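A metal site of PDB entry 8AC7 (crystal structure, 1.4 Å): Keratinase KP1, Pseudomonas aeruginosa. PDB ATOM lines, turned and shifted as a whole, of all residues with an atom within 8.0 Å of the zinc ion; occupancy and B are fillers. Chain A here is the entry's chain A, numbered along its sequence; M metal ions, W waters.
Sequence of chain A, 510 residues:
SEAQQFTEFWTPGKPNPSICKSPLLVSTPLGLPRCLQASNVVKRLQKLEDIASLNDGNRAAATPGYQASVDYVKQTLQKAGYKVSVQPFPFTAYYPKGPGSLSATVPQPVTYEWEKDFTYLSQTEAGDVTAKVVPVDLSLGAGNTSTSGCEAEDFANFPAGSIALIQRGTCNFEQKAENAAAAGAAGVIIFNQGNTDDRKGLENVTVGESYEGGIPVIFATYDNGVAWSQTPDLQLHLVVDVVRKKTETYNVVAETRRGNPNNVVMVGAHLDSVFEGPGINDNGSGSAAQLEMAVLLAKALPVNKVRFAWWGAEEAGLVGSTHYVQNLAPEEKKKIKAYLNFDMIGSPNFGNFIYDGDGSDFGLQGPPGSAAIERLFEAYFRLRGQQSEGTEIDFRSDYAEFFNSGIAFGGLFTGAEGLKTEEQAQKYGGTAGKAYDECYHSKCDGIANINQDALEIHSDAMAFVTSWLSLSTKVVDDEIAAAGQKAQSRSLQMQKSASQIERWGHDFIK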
ATOM      1  N   ILE A 354      16.347  -2.294 -27.089  1.00  0.00           N
ATOM      2  CA  ILE A 354      16.370  -3.494 -26.259  1.00  0.00           C
ATOM      3  C   ILE A 354      17.665  -4.245 -26.591  1.00  0.00           C
ATOM      4  O   ILE A 354      17.973  -4.448 -27.766  1.00  0.00           O
ATOM      5  CB  ILE A 354      15.143  -4.386 -26.555  1.00  0.00           C
ATOM      6  CG1 ILE A 354      13.848  -3.636 -26.198  1.00  0.00           C
ATOM      7  CG2 ILE A 354      15.256  -5.721 -25.817  1.00  0.00           C
ATOM      8  CD1 ILE A 354      12.581  -4.301 -26.758  1.00  0.00           C
ATOM      9  N   TYR A 355      18.409  -4.629 -25.562  1.00  0.00           N
ATOM     10  CA  TYR A 355      19.656  -5.372 -25.793  1.00  0.00           C
ATOM     11  C   TYR A 355      19.386  -6.555 -26.723  1.00  0.00           C
ATOM     12  O   TYR A 355      18.447  -7.332 -26.499  1.00  0.00           O
ATOM     13  CB  TYR A 355      20.226  -5.899 -24.479  1.00  0.00           C
ATOM     14  CG  TYR A 355      20.833  -4.877 -23.541  1.00  0.00           C
ATOM     15  CD1 TYR A 355      21.472  -5.296 -22.380  1.00  0.00           C
ATOM     16  CD2 TYR A 355      20.737  -3.511 -23.787  1.00  0.00           C
ATOM     17  CE1 TYR A 355      22.020  -4.391 -21.499  1.00  0.00           C
ATOM     18  CE2 TYR A 355      21.302  -2.578 -22.906  1.00  0.00           C
ATOM     19  CZ  TYR A 355      21.924  -3.040 -21.746  1.00  0.00           C
ATOM     20  OH  TYR A 355      22.490  -2.142 -20.854  1.00  0.00           O
ATOM     21  N   ASP A 356      20.242  -6.707 -27.727  1.00  0.00           N
ATOM     22  CA  ASP A 356      20.083  -7.736 -28.755  1.00  0.00           C
ATOM     23  C   ASP A 356      20.688  -9.066 -28.304  1.00  0.00           C
ATOM     24  O   ASP A 356      21.638  -9.587 -28.885  1.00  0.00           O
ATOM     25  CB  ASP A 356      20.715  -7.250 -30.060  1.00  0.00           C
ATOM     26  CG  ASP A 356      20.599  -8.259 -31.178  1.00  0.00           C
ATOM     27  OD1 ASP A 356      19.549  -8.927 -31.284  1.00  0.00           O
ATOM     28  OD2 ASP A 356      21.565  -8.364 -31.987  1.00  0.00           O
ATOM     29  N   GLY A 357      20.077  -9.631 -27.253  1.00  0.00           N
ATOM     30  CA  GLY A 357      20.600 -10.855 -26.671  1.00  0.00           C
ATOM     31  C   GLY A 357      20.596 -12.051 -27.595  1.00  0.00           C
ATOM     32  O   GLY A 357      21.379 -12.970 -27.398  1.00  0.00           O
ATOM     33  N   ASP A 358      19.717 -12.060 -28.603  1.00  0.00           N
ATOM     34  CA  ASP A 358      19.688 -13.155 -29.562  1.00  0.00           C
ATOM     35  C   ASP A 358      20.622 -12.977 -30.759  1.00  0.00           C
ATOM     36  O   ASP A 358      20.657 -13.850 -31.626  1.00  0.00           O
ATOM     37  CB  ASP A 358      18.248 -13.451 -30.034  1.00  0.00           C
ATOM     38  CG  ASP A 358      17.578 -12.258 -30.715  1.00  0.00           C
ATOM     39  OD1 ASP A 358      18.223 -11.211 -30.996  1.00  0.00           O
ATOM     40  OD2 ASP A 358      16.357 -12.360 -30.960  1.00  0.00           O
ATOM     41  N   GLY A 359      21.372 -11.877 -30.824  1.00  0.00           N
ATOM     42  CA  GLY A 359      22.249 -11.646 -31.959  1.00  0.00           C
ATOM     43  C   GLY A 359      21.548 -11.375 -33.266  1.00  0.00           C
ATOM     44  O   GLY A 359      22.200 -11.399 -34.313  1.00  0.00           O
ATOM     45  N   SER A 360      20.235 -11.117 -33.238  1.00  0.00           N
ATOM     46  CA  SER A 360      19.469 -10.978 -34.476  1.00  0.00           C
ATOM     47  C   SER A 360      19.903  -9.775 -35.306  1.00  0.00           C
ATOM     48  O   SER A 360      19.773  -9.801 -36.542  1.00  0.00           O
ATOM     49  CB  SER A 360      17.971 -10.913 -34.162  1.00  0.00           C
ATOM     50  OG  SER A 360      17.664  -9.746 -33.397  1.00  0.00           O
ATOM     51  N   ASP A 361      20.401  -8.723 -34.665  1.00  0.00           N
ATOM     52  CA  ASP A 361      20.827  -7.526 -35.381  1.00  0.00           C
ATOM     53  C   ASP A 361      22.327  -7.455 -35.589  1.00  0.00           C
ATOM     54  O   ASP A 361      22.777  -7.095 -36.674  1.00  0.00           O
ATOM     55  CB  ASP A 361      20.385  -6.268 -34.626  1.00  0.00           C
ATOM     56  CG  ASP A 361      18.888  -6.181 -34.466  1.00  0.00           C
ATOM     57  OD1 ASP A 361      18.169  -6.437 -35.457  1.00  0.00           O
ATOM     58  OD2 ASP A 361      18.439  -5.870 -33.341  1.00  0.00           O
ATOM     59  N   PHE A 362      23.116  -7.794 -34.576  1.00  0.00           N
ATOM     60  CA  PHE A 362      24.546  -7.549 -34.592  1.00  0.00           C
ATOM     61  C   PHE A 362      25.404  -8.794 -34.510  1.00  0.00           C
ATOM     62  O   PHE A 362      26.632  -8.684 -34.547  1.00  0.00           O
ATOM     63  CB  PHE A 362      24.939  -6.536 -33.508  1.00  0.00           C
ATOM     64  CG  PHE A 362      24.067  -5.311 -33.493  1.00  0.00           C
ATOM     65  CD1 PHE A 362      23.106  -5.131 -32.509  1.00  0.00           C
ATOM     66  CD2 PHE A 362      24.209  -4.322 -34.467  1.00  0.00           C
ATOM     67  CE1 PHE A 362      22.299  -4.018 -32.494  1.00  0.00           C
ATOM     68  CE2 PHE A 362      23.402  -3.196 -34.452  1.00  0.00           C
ATOM     69  CZ  PHE A 362      22.436  -3.052 -33.449  1.00  0.00           C
ATOM     70  N   GLY A 363      24.812  -9.980 -34.406  1.00  0.00           N
ATOM     71  CA  GLY A 363      25.548 -11.215 -34.499  1.00  0.00           C
ATOM     72  C   GLY A 363      26.198 -11.705 -33.214  1.00  0.00           C
ATOM     73  O   GLY A 363      26.802 -12.777 -33.228  1.00  0.00           O
ATOM     74  N   LEU A 364      26.085 -10.966 -32.119  1.00  0.00           N
ATOM     75  CA  LEU A 364      26.670 -11.363 -30.848  1.00  0.00           C
ATOM     76  C   LEU A 364      25.533 -11.824 -29.945  1.00  0.00           C
ATOM     77  O   LEU A 364      24.593 -11.074 -29.679  1.00  0.00           O
ATOM     78  CB  LEU A 364      27.415 -10.189 -30.205  1.00  0.00           C
ATOM     79  CG  LEU A 364      28.037 -10.450 -28.830  1.00  0.00           C
ATOM     80  CD1 LEU A 364      28.999 -11.637 -28.891  1.00  0.00           C
ATOM     81  CD2 LEU A 364      28.755  -9.199 -28.297  1.00  0.00           C
ATOM     82  N   SER A 370      19.372 -15.292 -22.589  1.00  0.00           N
ATOM     83  CA  SER A 370      19.334 -13.904 -22.999  1.00  0.00           C
ATOM     84  C   SER A 370      18.311 -13.660 -24.099  1.00  0.00           C
ATOM     85  O   SER A 370      17.659 -12.608 -24.130  1.00  0.00           O
ATOM     86  CB  SER A 370      20.725 -13.411 -23.410  1.00  0.00           C
ATOM     87  OG  SER A 370      21.709 -13.733 -22.435  1.00  0.00           O
ATOM     88  N   ALA A 371      18.155 -14.624 -25.026  1.00  0.00           N
ATOM     89  CA  ALA A 371      17.119 -14.477 -26.045  1.00  0.00           C
ATOM     90  C   ALA A 371      15.742 -14.365 -25.409  1.00  0.00           C
ATOM     91  O   ALA A 371      14.929 -13.528 -25.810  1.00  0.00           O
ATOM     92  CB  ALA A 371      17.170 -15.633 -27.038  1.00  0.00           C
ATOM     93  N   GLU A 374      15.260 -10.875 -23.890  1.00  0.00           N
ATOM     94  CA  GLU A 374      15.018  -9.919 -24.963  1.00  0.00           C
ATOM     95  C   GLU A 374      13.597 -10.043 -25.485  1.00  0.00           C
ATOM     96  O   GLU A 374      12.932  -9.028 -25.742  1.00  0.00           O
ATOM     97  CB  GLU A 374      16.038 -10.148 -26.092  1.00  0.00           C
ATOM     98  CG  GLU A 374      15.848  -9.296 -27.328  1.00  0.00           C
ATOM     99  CD  GLU A 374      16.772  -9.710 -28.446  1.00  0.00           C
ATOM    100  OE1 GLU A 374      17.299 -10.829 -28.370  1.00  0.00           O
ATOM    101  OE2 GLU A 374      16.957  -8.934 -29.417  1.00  0.00           O
ATOM    102  N   ARG A 375      13.117 -11.277 -25.645  1.00  0.00           N
ATOM    103  CA  ARG A 375      11.783 -11.497 -26.199  1.00  0.00           C
ATOM    104  C   ARG A 375      10.695 -10.967 -25.277  1.00  0.00           C
ATOM    105  O   ARG A 375       9.680 -10.439 -25.744  1.00  0.00           O
ATOM    106  CB  ARG A 375      11.567 -12.985 -26.476  1.00  0.00           C
ATOM    107  CG  ARG A 375      10.472 -13.285 -27.489  1.00  0.00           C
ATOM    108  CD  ARG A 375      10.477 -14.750 -27.896  1.00  0.00           C
ATOM    109  NE  ARG A 375       9.355 -15.464 -27.285  1.00  0.00           N
ATOM    110  CZ  ARG A 375       8.613 -16.355 -27.921  1.00  0.00           C
ATOM    111  NH1 ARG A 375       7.612 -16.957 -27.284  1.00  0.00           N
ATOM    112  NH2 ARG A 375       8.861 -16.653 -29.189  1.00  0.00           N
ATOM    113  N   GLU A 378      10.624  -7.324 -25.863  1.00  0.00           N
ATOM    114  CA  GLU A 378      10.073  -7.065 -27.192  1.00  0.00           C
ATOM    115  C   GLU A 378       8.561  -7.240 -27.177  1.00  0.00           C
ATOM    116  O   GLU A 378       7.823  -6.421 -27.745  1.00  0.00           O
ATOM    117  CB  GLU A 378      10.704  -8.010 -28.222  1.00  0.00           C
ATOM    118  CG  GLU A 378      12.144  -7.675 -28.586  1.00  0.00           C
ATOM    119  CD  GLU A 378      12.796  -8.758 -29.421  1.00  0.00           C
ATOM    120  OE1 GLU A 378      13.840  -8.462 -30.047  1.00  0.00           O
ATOM    121  OE2 GLU A 378      12.279  -9.900 -29.468  1.00  0.00           O
ATOM    122  N   GLU A 389      13.769  -1.620 -31.114  1.00  0.00           N
ATOM    123  CA  GLU A 389      14.784  -2.210 -31.980  1.00  0.00           C
ATOM    124  C   GLU A 389      15.996  -2.587 -31.135  1.00  0.00           C
ATOM    125  O   GLU A 389      16.124  -2.174 -29.984  1.00  0.00           O
ATOM    126  CB  GLU A 389      15.169  -1.288 -33.134  1.00  0.00           C
ATOM    127  CG  GLU A 389      15.895  -0.024 -32.703  1.00  0.00           C
ATOM    128  CD  GLU A 389      15.962   0.986 -33.820  1.00  0.00           C
ATOM    129  OE1 GLU A 389      17.025   1.072 -34.483  1.00  0.00           O
ATOM    130  OE2 GLU A 389      14.948   1.671 -34.050  1.00  0.00           O
ATOM    131  N   GLY A 390      16.883  -3.362 -31.736  1.00  0.00           N
ATOM    132  CA  GLY A 390      18.033  -3.867 -31.022  1.00  0.00           C
ATOM    133  C   GLY A 390      19.123  -2.829 -30.820  1.00  0.00           C
ATOM    134  O   GLY A 390      19.250  -1.847 -31.553  1.00  0.00           O
ATOM    135  N   THR A 391      19.912  -3.057 -29.776  1.00  0.00           N
ATOM    136  CA  THR A 391      21.155  -2.337 -29.576  1.00  0.00           C
ATOM    137  C   THR A 391      22.251  -3.327 -29.202  1.00  0.00           C
ATOM    138  O   THR A 391      21.977  -4.431 -28.729  1.00  0.00           O
ATOM    139  CB  THR A 391      20.978  -1.219 -28.536  1.00  0.00           C
ATOM    140  OG1 THR A 391      22.113  -0.352 -28.566  1.00  0.00           O
ATOM    141  CG2 THR A 391      20.818  -1.799 -27.142  1.00  0.00           C
HETATM  142 ZN    ZN M   1      17.555  -9.366 -31.278  1.00  0.00          ZN
HETATM  143  O   HOH W   1      16.957  -7.518 -31.873  1.00  0.00           O
HETATM  144  O   HOH W   2      15.456 -10.071 -31.500  1.00  0.00           O
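The zinc ion is bound by the side-chain carboxylate (OD1) of Asp 358 (2.0 Å), the side-chain carboxylate (OE2) of Glu 374 (2.0 Å), water W1 (2.0 Å), the side-chain carboxylate (OD1) of Asp 356 (2.0 Å), the side-chain hydroxyl (OG) of Ser 360 (2.2 Å) and water W2 (2.2 Å).
Of the 19 residues printed, 4 come within 4 Å of the zinc ion.
The nearest printed residue that does not touch the zinc ion is Glu 378 (4.02 Å).
The backbone NH (N) of Gly 357 lies within hydrogen-bond range of the side-chain carboxylate (OE1) of Glu 374 (3.2 Å).
The side-chain carboxylate (OD2) of Asp 356 lies within hydrogen-bond range of the backbone NH (N) of Asp 361.
N of Gly 359 lies close to OD1 of Asp 356.
The side-chain carboxylate (OD2) of Asp 356 is in hydrogen-bond range of the backbone NH (N) of Phe 362 (3.1 Å).
N of Asp 356 sits at hydrogen-bond distance from O of Thr 391 (3.0 Å).
Water W2 lies within hydrogen-bond range of the side-chain carboxylate (OD2) of Asp 358 and the side-chain carboxylate (OE1) of Glu 378.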
